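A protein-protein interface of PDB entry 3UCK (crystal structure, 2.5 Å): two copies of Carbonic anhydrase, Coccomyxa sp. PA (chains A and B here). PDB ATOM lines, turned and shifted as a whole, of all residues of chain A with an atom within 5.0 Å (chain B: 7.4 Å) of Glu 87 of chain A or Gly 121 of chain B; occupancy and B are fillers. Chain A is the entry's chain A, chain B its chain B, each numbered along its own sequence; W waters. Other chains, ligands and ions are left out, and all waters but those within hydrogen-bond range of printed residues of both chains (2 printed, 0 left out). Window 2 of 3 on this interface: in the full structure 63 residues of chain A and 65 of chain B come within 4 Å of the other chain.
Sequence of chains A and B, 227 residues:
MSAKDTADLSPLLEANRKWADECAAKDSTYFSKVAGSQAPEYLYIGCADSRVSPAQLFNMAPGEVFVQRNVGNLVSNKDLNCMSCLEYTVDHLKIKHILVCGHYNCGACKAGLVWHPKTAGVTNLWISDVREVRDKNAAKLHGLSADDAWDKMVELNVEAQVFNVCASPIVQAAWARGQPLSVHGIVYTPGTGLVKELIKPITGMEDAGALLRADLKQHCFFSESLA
OG of Ser 84 of chain A lies within hydrogen-bond range of OG1 of Thr 123 of chain B (3.1 Å). N of Thr 123 of chain B sits at hydrogen-bond distance from OE1 of Glu 87 of chain A, at 3.1 Å. The side-chain carboxylate (OE2) of Glu 87 of chain A lies within hydrogen-bond range of the backbone NH (N) of Val 122 of chain B, at 2.7 Å.
O of Met 83 of chain A touches CG2 of Val 122 of chain B, 3.7 Å away. OG of Ser 84 of chain A touches CB of Trp 126 of chain B, at 3.6 Å. CA of Gly 121 of chain B touches OE2 of Glu 87 of chain A, 3.1 Å away. OG1 of Thr 123 of chain B touches N of Tyr 88 of chain A, at 3.96 Å.
Of chain B, only Gly 121 (3.1 Å), Val 122 (2.7 Å) and Thr 123 (3.1 Å) come within 4 Å of Glu 87 of chain A. Gly 121 of chain B touches just one residue of chain A: Glu 87. Printed residues of chain A within 4 Å of Trp 126 of chain B: Ser 84 (3.6 Å). Printed residues of chain B within 4 Å of Ser 84 of chain A: Thr 123 (3.1 Å) and Trp 126 (3.6 Å). Of the printed residues of chain B, Tyr 88 of chain A touches Thr 123 (3.96 Å). Of the printed residues of chain A, Thr 123 of chain B touches Ser 84, Glu 87 and Tyr 88. Ala 120 of chain B touches none of the printed residues of chain A. Thr 89 of chain A touches none of the printed residues of chain B. The nearest residue of chain B that does not touch Glu 87 of chain A is Ala 120 of chain B (4.6 Å). The nearest printed residue of chain A that does not touch Trp 126 of chain B is Cys 85 of chain A (6.6 Å).
Hydrophobic or aromatic side chains of chain B within 4 Å of the printed part of chain A: Val 122 and Trp 126. Along chain B the printed residues that touch a printed residue of chain A span positions 121 to 126. Hydrophobic or aromatic side chains of chain A within 4 Å of the printed part of chain B: Tyr 88. Among the printed residues, 7 pairs touch across the chains.
No position is printed for both chains.
Water W1 lies within hydrogen-bond range of the backbone carbonyl oxygen of Ala 120 of chain B, the side-chain carboxylate of Glu 87 of chain A, the backbone NH of Asn 124 of chain B and the backbone NH of Thr 123 of chain B. Water W2 lies within hydrogen-bond range of OE1 of Glu 87 of chain A (2.8 Å), OG1 of Thr 123 of chain B (2.9 Å), NE2 of His 92 of chain A (3.1 Å) and N of Tyr 88 of chain A (3.4 Å).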
ATOM      1  N   MET A  83       7.846 -22.327  29.094  1.00  0.00           N
ATOM      2  CA  MET A  83       8.731 -21.285  28.711  1.00  0.00           C
ATOM      3  C   MET A  83       8.056 -19.951  28.872  1.00  0.00           C
ATOM      4  O   MET A  83       8.726 -18.968  29.113  1.00  0.00           O
ATOM      5  CB  MET A  83       9.170 -21.509  27.303  1.00  0.00           C
ATOM      6  CG  MET A  83      10.109 -22.636  27.248  1.00  0.00           C
ATOM      7  SD  MET A  83      11.688 -22.000  27.732  1.00  0.00           S
ATOM      8  CE  MET A  83      11.946 -22.918  29.236  1.00  0.00           C
ATOM      9  N   SER A  84       6.732 -19.933  28.817  1.00  0.00           N
ATOM     10  CA  SER A  84       5.969 -18.744  29.107  1.00  0.00           C
ATOM     11  C   SER A  84       6.008 -18.286  30.582  1.00  0.00           C
ATOM     12  O   SER A  84       6.145 -17.101  30.870  1.00  0.00           O
ATOM     13  CB  SER A  84       4.552 -18.991  28.737  1.00  0.00           C
ATOM     14  OG  SER A  84       3.995 -17.791  28.340  1.00  0.00           O
ATOM     15  N   CYS A  85       5.792 -19.213  31.506  1.00  0.00           N
ATOM     16  CA  CYS A  85       6.000 -18.952  32.913  1.00  0.00           C
ATOM     17  C   CYS A  85       7.413 -18.470  33.112  1.00  0.00           C
ATOM     18  O   CYS A  85       7.645 -17.566  33.897  1.00  0.00           O
ATOM     19  CB  CYS A  85       5.779 -20.218  33.717  1.00  0.00           C
ATOM     20  SG  CYS A  85       4.090 -20.884  33.594  1.00  0.00           S
ATOM     21  N   LEU A  86       8.372 -19.052  32.385  1.00  0.00           N
ATOM     22  CA  LEU A  86       9.747 -18.640  32.567  1.00  0.00           C
ATOM     23  C   LEU A  86       9.985 -17.196  32.044  1.00  0.00           C
ATOM     24  O   LEU A  86      10.523 -16.373  32.792  1.00  0.00           O
ATOM     25  CB  LEU A  86      10.714 -19.642  31.965  1.00  0.00           C
ATOM     26  CG  LEU A  86      12.221 -19.511  32.271  1.00  0.00           C
ATOM     27  CD1 LEU A  86      12.692 -19.765  33.712  1.00  0.00           C
ATOM     28  CD2 LEU A  86      12.881 -20.509  31.373  1.00  0.00           C
ATOM     29  N   GLU A  87       9.614 -16.933  30.785  1.00  0.00           N
ATOM     30  CA  GLU A  87       9.832 -15.638  30.144  1.00  0.00           C
ATOM     31  C   GLU A  87       9.204 -14.543  30.999  1.00  0.00           C
ATOM     32  O   GLU A  87       9.877 -13.612  31.422  1.00  0.00           O
ATOM     33  CB  GLU A  87       9.185 -15.590  28.770  1.00  0.00           C
ATOM     34  CG  GLU A  87       9.546 -14.376  28.027  1.00  0.00           C
ATOM     35  CD  GLU A  87       8.860 -14.226  26.709  1.00  0.00           C
ATOM     36  OE1 GLU A  87       7.738 -13.700  26.674  1.00  0.00           O
ATOM     37  OE2 GLU A  87       9.449 -14.536  25.658  1.00  0.00           O
ATOM     38  N   TYR A  88       7.918 -14.698  31.296  1.00  0.00           N
ATOM     39  CA  TYR A  88       7.163 -13.733  32.053  1.00  0.00           C
ATOM     40  C   TYR A  88       7.743 -13.314  33.437  1.00  0.00           C
ATOM     41  O   TYR A  88       7.621 -12.170  33.859  1.00  0.00           O
ATOM     42  CB  TYR A  88       5.749 -14.263  32.281  1.00  0.00           C
ATOM     43  CG  TYR A  88       4.838 -13.189  32.781  1.00  0.00           C
ATOM     44  CD1 TYR A  88       4.554 -12.074  31.985  1.00  0.00           C
ATOM     45  CD2 TYR A  88       4.271 -13.264  34.061  1.00  0.00           C
ATOM     46  CE1 TYR A  88       3.716 -11.052  32.445  1.00  0.00           C
ATOM     47  CE2 TYR A  88       3.424 -12.275  34.521  1.00  0.00           C
ATOM     48  CZ  TYR A  88       3.153 -11.163  33.697  1.00  0.00           C
ATOM     49  OH  TYR A  88       2.305 -10.163  34.128  1.00  0.00           O
ATOM     50  N   THR A  89       8.301 -14.268  34.159  1.00  0.00           N
ATOM     51  CA  THR A  89       8.719 -14.001  35.480  1.00  0.00           C
ATOM     52  C   THR A  89      10.111 -13.446  35.452  1.00  0.00           C
ATOM     53  O   THR A  89      10.433 -12.637  36.315  1.00  0.00           O
ATOM     54  CB  THR A  89       8.672 -15.219  36.337  1.00  0.00           C
ATOM     55  OG1 THR A  89       9.473 -16.228  35.742  1.00  0.00           O
ATOM     56  CG2 THR A  89       7.222 -15.666  36.482  1.00  0.00           C
ATOM     57  N   VAL A  90      10.920 -13.857  34.477  1.00  0.00           N
ATOM     58  CA  VAL A  90      12.253 -13.321  34.384  1.00  0.00           C
ATOM     59  C   VAL A  90      12.226 -11.908  33.739  1.00  0.00           C
ATOM     60  O   VAL A  90      12.737 -10.962  34.303  1.00  0.00           O
ATOM     61  CB  VAL A  90      13.221 -14.283  33.674  1.00  0.00           C
ATOM     62  CG1 VAL A  90      14.427 -13.586  33.143  1.00  0.00           C
ATOM     63  CG2 VAL A  90      13.640 -15.401  34.626  1.00  0.00           C
ATOM     64  N   ASP A  91      11.626 -11.786  32.572  1.00  0.00           N
ATOM     65  CA  ASP A  91      11.630 -10.565  31.854  1.00  0.00           C
ATOM     66  C   ASP A  91      10.697  -9.485  32.420  1.00  0.00           C
ATOM     67  O   ASP A  91      11.102  -8.288  32.460  1.00  0.00           O
ATOM     68  CB  ASP A  91      11.301 -10.820  30.402  1.00  0.00           C
ATOM     69  CG  ASP A  91      12.375 -11.595  29.704  1.00  0.00           C
ATOM     70  OD1 ASP A  91      13.341 -12.068  30.377  1.00  0.00           O
ATOM     71  OD2 ASP A  91      12.262 -11.725  28.464  1.00  0.00           O
ATOM     72  N   HIS A  92       9.484  -9.867  32.843  1.00  0.00           N
ATOM     73  CA  HIS A  92       8.491  -8.885  33.242  1.00  0.00           C
ATOM     74  C   HIS A  92       8.410  -8.735  34.771  1.00  0.00           C
ATOM     75  O   HIS A  92       8.599  -7.671  35.294  1.00  0.00           O
ATOM     76  CB  HIS A  92       7.125  -9.185  32.587  1.00  0.00           C
ATOM     77  CG  HIS A  92       7.129  -9.121  31.078  1.00  0.00           C
ATOM     78  ND1 HIS A  92       7.458  -7.979  30.373  1.00  0.00           N
ATOM     79  CD2 HIS A  92       6.796 -10.050  30.145  1.00  0.00           C
ATOM     80  CE1 HIS A  92       7.341  -8.213  29.075  1.00  0.00           C
ATOM     81  NE2 HIS A  92       6.952  -9.464  28.908  1.00  0.00           N
ATOM     82  N   ILE A 170      15.972 -17.747  27.963  1.00  0.00           N
ATOM     83  CA  ILE A 170      15.457 -16.705  28.838  1.00  0.00           C
ATOM     84  C   ILE A 170      16.503 -16.469  29.904  1.00  0.00           C
ATOM     85  O   ILE A 170      16.930 -15.300  30.092  1.00  0.00           O
ATOM     86  CB  ILE A 170      14.179 -17.111  29.616  1.00  0.00           C
ATOM     87  CG1 ILE A 170      13.076 -17.698  28.697  1.00  0.00           C
ATOM     88  CG2 ILE A 170      13.690 -15.987  30.429  1.00  0.00           C
ATOM     89  CD1 ILE A 170      12.594 -16.773  27.566  1.00  0.00           C
ATOM     90  N   TRP B 115      -2.002  -6.278  23.963  1.00  0.00           N
ATOM     91  CA  TRP B 115      -0.873  -6.470  23.045  1.00  0.00           C
ATOM     92  C   TRP B 115      -1.208  -6.526  21.571  1.00  0.00           C
ATOM     93  O   TRP B 115      -2.315  -6.929  21.145  1.00  0.00           O
ATOM     94  CB  TRP B 115      -0.054  -7.678  23.409  1.00  0.00           C
ATOM     95  CG  TRP B 115       0.497  -7.643  24.744  1.00  0.00           C
ATOM     96  CD1 TRP B 115       0.289  -6.685  25.686  1.00  0.00           C
ATOM     97  CD2 TRP B 115       1.312  -8.644  25.351  1.00  0.00           C
ATOM     98  NE1 TRP B 115       0.974  -7.002  26.837  1.00  0.00           N
ATOM     99  CE2 TRP B 115       1.613  -8.198  26.661  1.00  0.00           C
ATOM    100  CE3 TRP B 115       1.846  -9.869  24.909  1.00  0.00           C
ATOM    101  CZ2 TRP B 115       2.409  -8.939  27.551  1.00  0.00           C
ATOM    102  CZ3 TRP B 115       2.648 -10.613  25.793  1.00  0.00           C
ATOM    103  CH2 TRP B 115       2.924 -10.139  27.099  1.00  0.00           C
ATOM    104  N   PRO B 117      -0.279  -8.345  18.207  1.00  0.00           N
ATOM    105  CA  PRO B 117       0.210  -9.672  17.925  1.00  0.00           C
ATOM    106  C   PRO B 117       1.672  -9.681  17.616  1.00  0.00           C
ATOM    107  O   PRO B 117       2.247 -10.728  17.619  1.00  0.00           O
ATOM    108  CB  PRO B 117      -0.545 -10.036  16.667  1.00  0.00           C
ATOM    109  CG  PRO B 117      -1.721  -9.288  16.714  1.00  0.00           C
ATOM    110  CD  PRO B 117      -1.429  -8.018  17.369  1.00  0.00           C
ATOM    111  N   LYS B 118       2.274  -8.549  17.330  1.00  0.00           N
ATOM    112  CA  LYS B 118       3.646  -8.578  16.889  1.00  0.00           C
ATOM    113  C   LYS B 118       4.596  -8.545  18.036  1.00  0.00           C
ATOM    114  O   LYS B 118       5.745  -8.826  17.882  1.00  0.00           O
ATOM    115  CB  LYS B 118       3.931  -7.442  15.943  1.00  0.00           C
ATOM    116  CG  LYS B 118       4.112  -6.141  16.631  1.00  0.00           C
ATOM    117  CD  LYS B 118       4.390  -5.063  15.660  1.00  0.00           C
ATOM    118  CE  LYS B 118       4.594  -3.799  16.354  1.00  0.00           C
ATOM    119  NZ  LYS B 118       3.529  -2.899  15.989  1.00  0.00           N
ATOM    120  N   THR B 119       4.106  -8.217  19.204  1.00  0.00           N
ATOM    121  CA  THR B 119       4.948  -8.236  20.355  1.00  0.00           C
ATOM    122  C   THR B 119       5.823  -9.436  20.233  1.00  0.00           C
ATOM    123  O   THR B 119       5.487 -10.360  19.574  1.00  0.00           O
ATOM    124  CB  THR B 119       4.129  -8.372  21.568  1.00  0.00           C
ATOM    125  OG1 THR B 119       3.125  -7.380  21.526  1.00  0.00           O
ATOM    126  CG2 THR B 119       4.956  -8.151  22.750  1.00  0.00           C
ATOM    127  N   ALA B 120       6.961  -9.434  20.874  1.00  0.00           N
ATOM    128  CA  ALA B 120       7.865 -10.523  20.689  1.00  0.00           C
ATOM    129  C   ALA B 120       7.882 -11.405  21.887  1.00  0.00           C
ATOM    130  O   ALA B 120       7.403 -11.045  22.925  1.00  0.00           O
ATOM    131  CB  ALA B 120       9.211 -10.009  20.426  1.00  0.00           C
ATOM    132  N   GLY B 121       8.452 -12.576  21.738  1.00  0.00           N
ATOM    133  CA  GLY B 121       8.532 -13.473  22.854  1.00  0.00           C
ATOM    134  C   GLY B 121       7.538 -14.590  22.842  1.00  0.00           C
ATOM    135  O   GLY B 121       6.677 -14.645  22.017  1.00  0.00           O
ATOM    136  N   VAL B 122       7.691 -15.480  23.795  1.00  0.00           N
ATOM    137  CA  VAL B 122       6.908 -16.682  23.834  1.00  0.00           C
ATOM    138  C   VAL B 122       5.616 -16.461  24.546  1.00  0.00           C
ATOM    139  O   VAL B 122       4.613 -16.953  24.138  1.00  0.00           O
ATOM    140  CB  VAL B 122       7.665 -17.823  24.454  1.00  0.00           C
ATOM    141  CG1 VAL B 122       8.872 -18.087  23.672  1.00  0.00           C
ATOM    142  CG2 VAL B 122       8.043 -17.494  25.808  1.00  0.00           C
ATOM    143  N   THR B 123       5.626 -15.692  25.605  1.00  0.00           N
ATOM    144  CA  THR B 123       4.350 -15.349  26.184  1.00  0.00           C
ATOM    145  C   THR B 123       3.279 -14.943  25.164  1.00  0.00           C
ATOM    146  O   THR B 123       2.136 -15.471  25.192  1.00  0.00           O
ATOM    147  CB  THR B 123       4.460 -14.389  27.344  1.00  0.00           C
ATOM    148  OG1 THR B 123       5.260 -14.979  28.377  1.00  0.00           O
ATOM    149  CG2 THR B 123       3.072 -14.167  27.937  1.00  0.00           C
ATOM    150  N   ASN B 124       3.630 -14.039  24.269  1.00  0.00           N
ATOM    151  CA  ASN B 124       2.705 -13.506  23.290  1.00  0.00           C
ATOM    152  C   ASN B 124       2.160 -14.602  22.384  1.00  0.00           C
ATOM    153  O   ASN B 124       1.018 -14.570  21.974  1.00  0.00           O
ATOM    154  CB  ASN B 124       3.383 -12.439  22.400  1.00  0.00           C
ATOM    155  CG  ASN B 124       2.480 -11.977  21.295  1.00  0.00           C
ATOM    156  OD1 ASN B 124       1.432 -11.356  21.557  1.00  0.00           O
ATOM    157  ND2 ASN B 124       2.818 -12.323  20.065  1.00  0.00           N
ATOM    158  N   LEU B 125       3.015 -15.539  22.022  1.00  0.00           N
ATOM    159  CA  LEU B 125       2.645 -16.712  21.232  1.00  0.00           C
ATOM    160  C   LEU B 125       1.654 -17.535  22.053  1.00  0.00           C
ATOM    161  O   LEU B 125       0.509 -17.799  21.550  1.00  0.00           O
ATOM    162  CB  LEU B 125       3.896 -17.542  20.943  1.00  0.00           C
ATOM    163  CG  LEU B 125       4.950 -17.017  19.954  1.00  0.00           C
ATOM    164  CD1 LEU B 125       6.101 -18.038  19.810  1.00  0.00           C
ATOM    165  CD2 LEU B 125       4.327 -16.743  18.574  1.00  0.00           C
ATOM    166  N   TRP B 126       2.053 -17.845  23.328  1.00  0.00           N
ATOM    167  CA  TRP B 126       1.262 -18.657  24.252  1.00  0.00           C
ATOM    168  C   TRP B 126      -0.124 -18.100  24.500  1.00  0.00           C
ATOM    169  O   TRP B 126      -1.091 -18.837  24.617  1.00  0.00           O
ATOM    170  CB  TRP B 126       1.926 -18.776  25.615  1.00  0.00           C
ATOM    171  CG  TRP B 126       1.105 -19.578  26.634  1.00  0.00           C
ATOM    172  CD1 TRP B 126       0.440 -19.104  27.641  1.00  0.00           C
ATOM    173  CD2 TRP B 126       0.880 -21.007  26.629  1.00  0.00           C
ATOM    174  NE1 TRP B 126      -0.203 -20.118  28.348  1.00  0.00           N
ATOM    175  CE2 TRP B 126       0.085 -21.305  27.739  1.00  0.00           C
ATOM    176  CE3 TRP B 126       1.322 -22.062  25.801  1.00  0.00           C
ATOM    177  CZ2 TRP B 126      -0.300 -22.627  28.084  1.00  0.00           C
ATOM    178  CZ3 TRP B 126       0.894 -23.411  26.123  1.00  0.00           C
ATOM    179  CH2 TRP B 126       0.093 -23.650  27.255  1.00  0.00           C
HETATM  180  O   HOH W   1       6.000 -12.384  24.763  1.00  0.00           O
HETATM  181  O   HOH W   2       6.653 -12.553  28.952  1.00  0.00           O
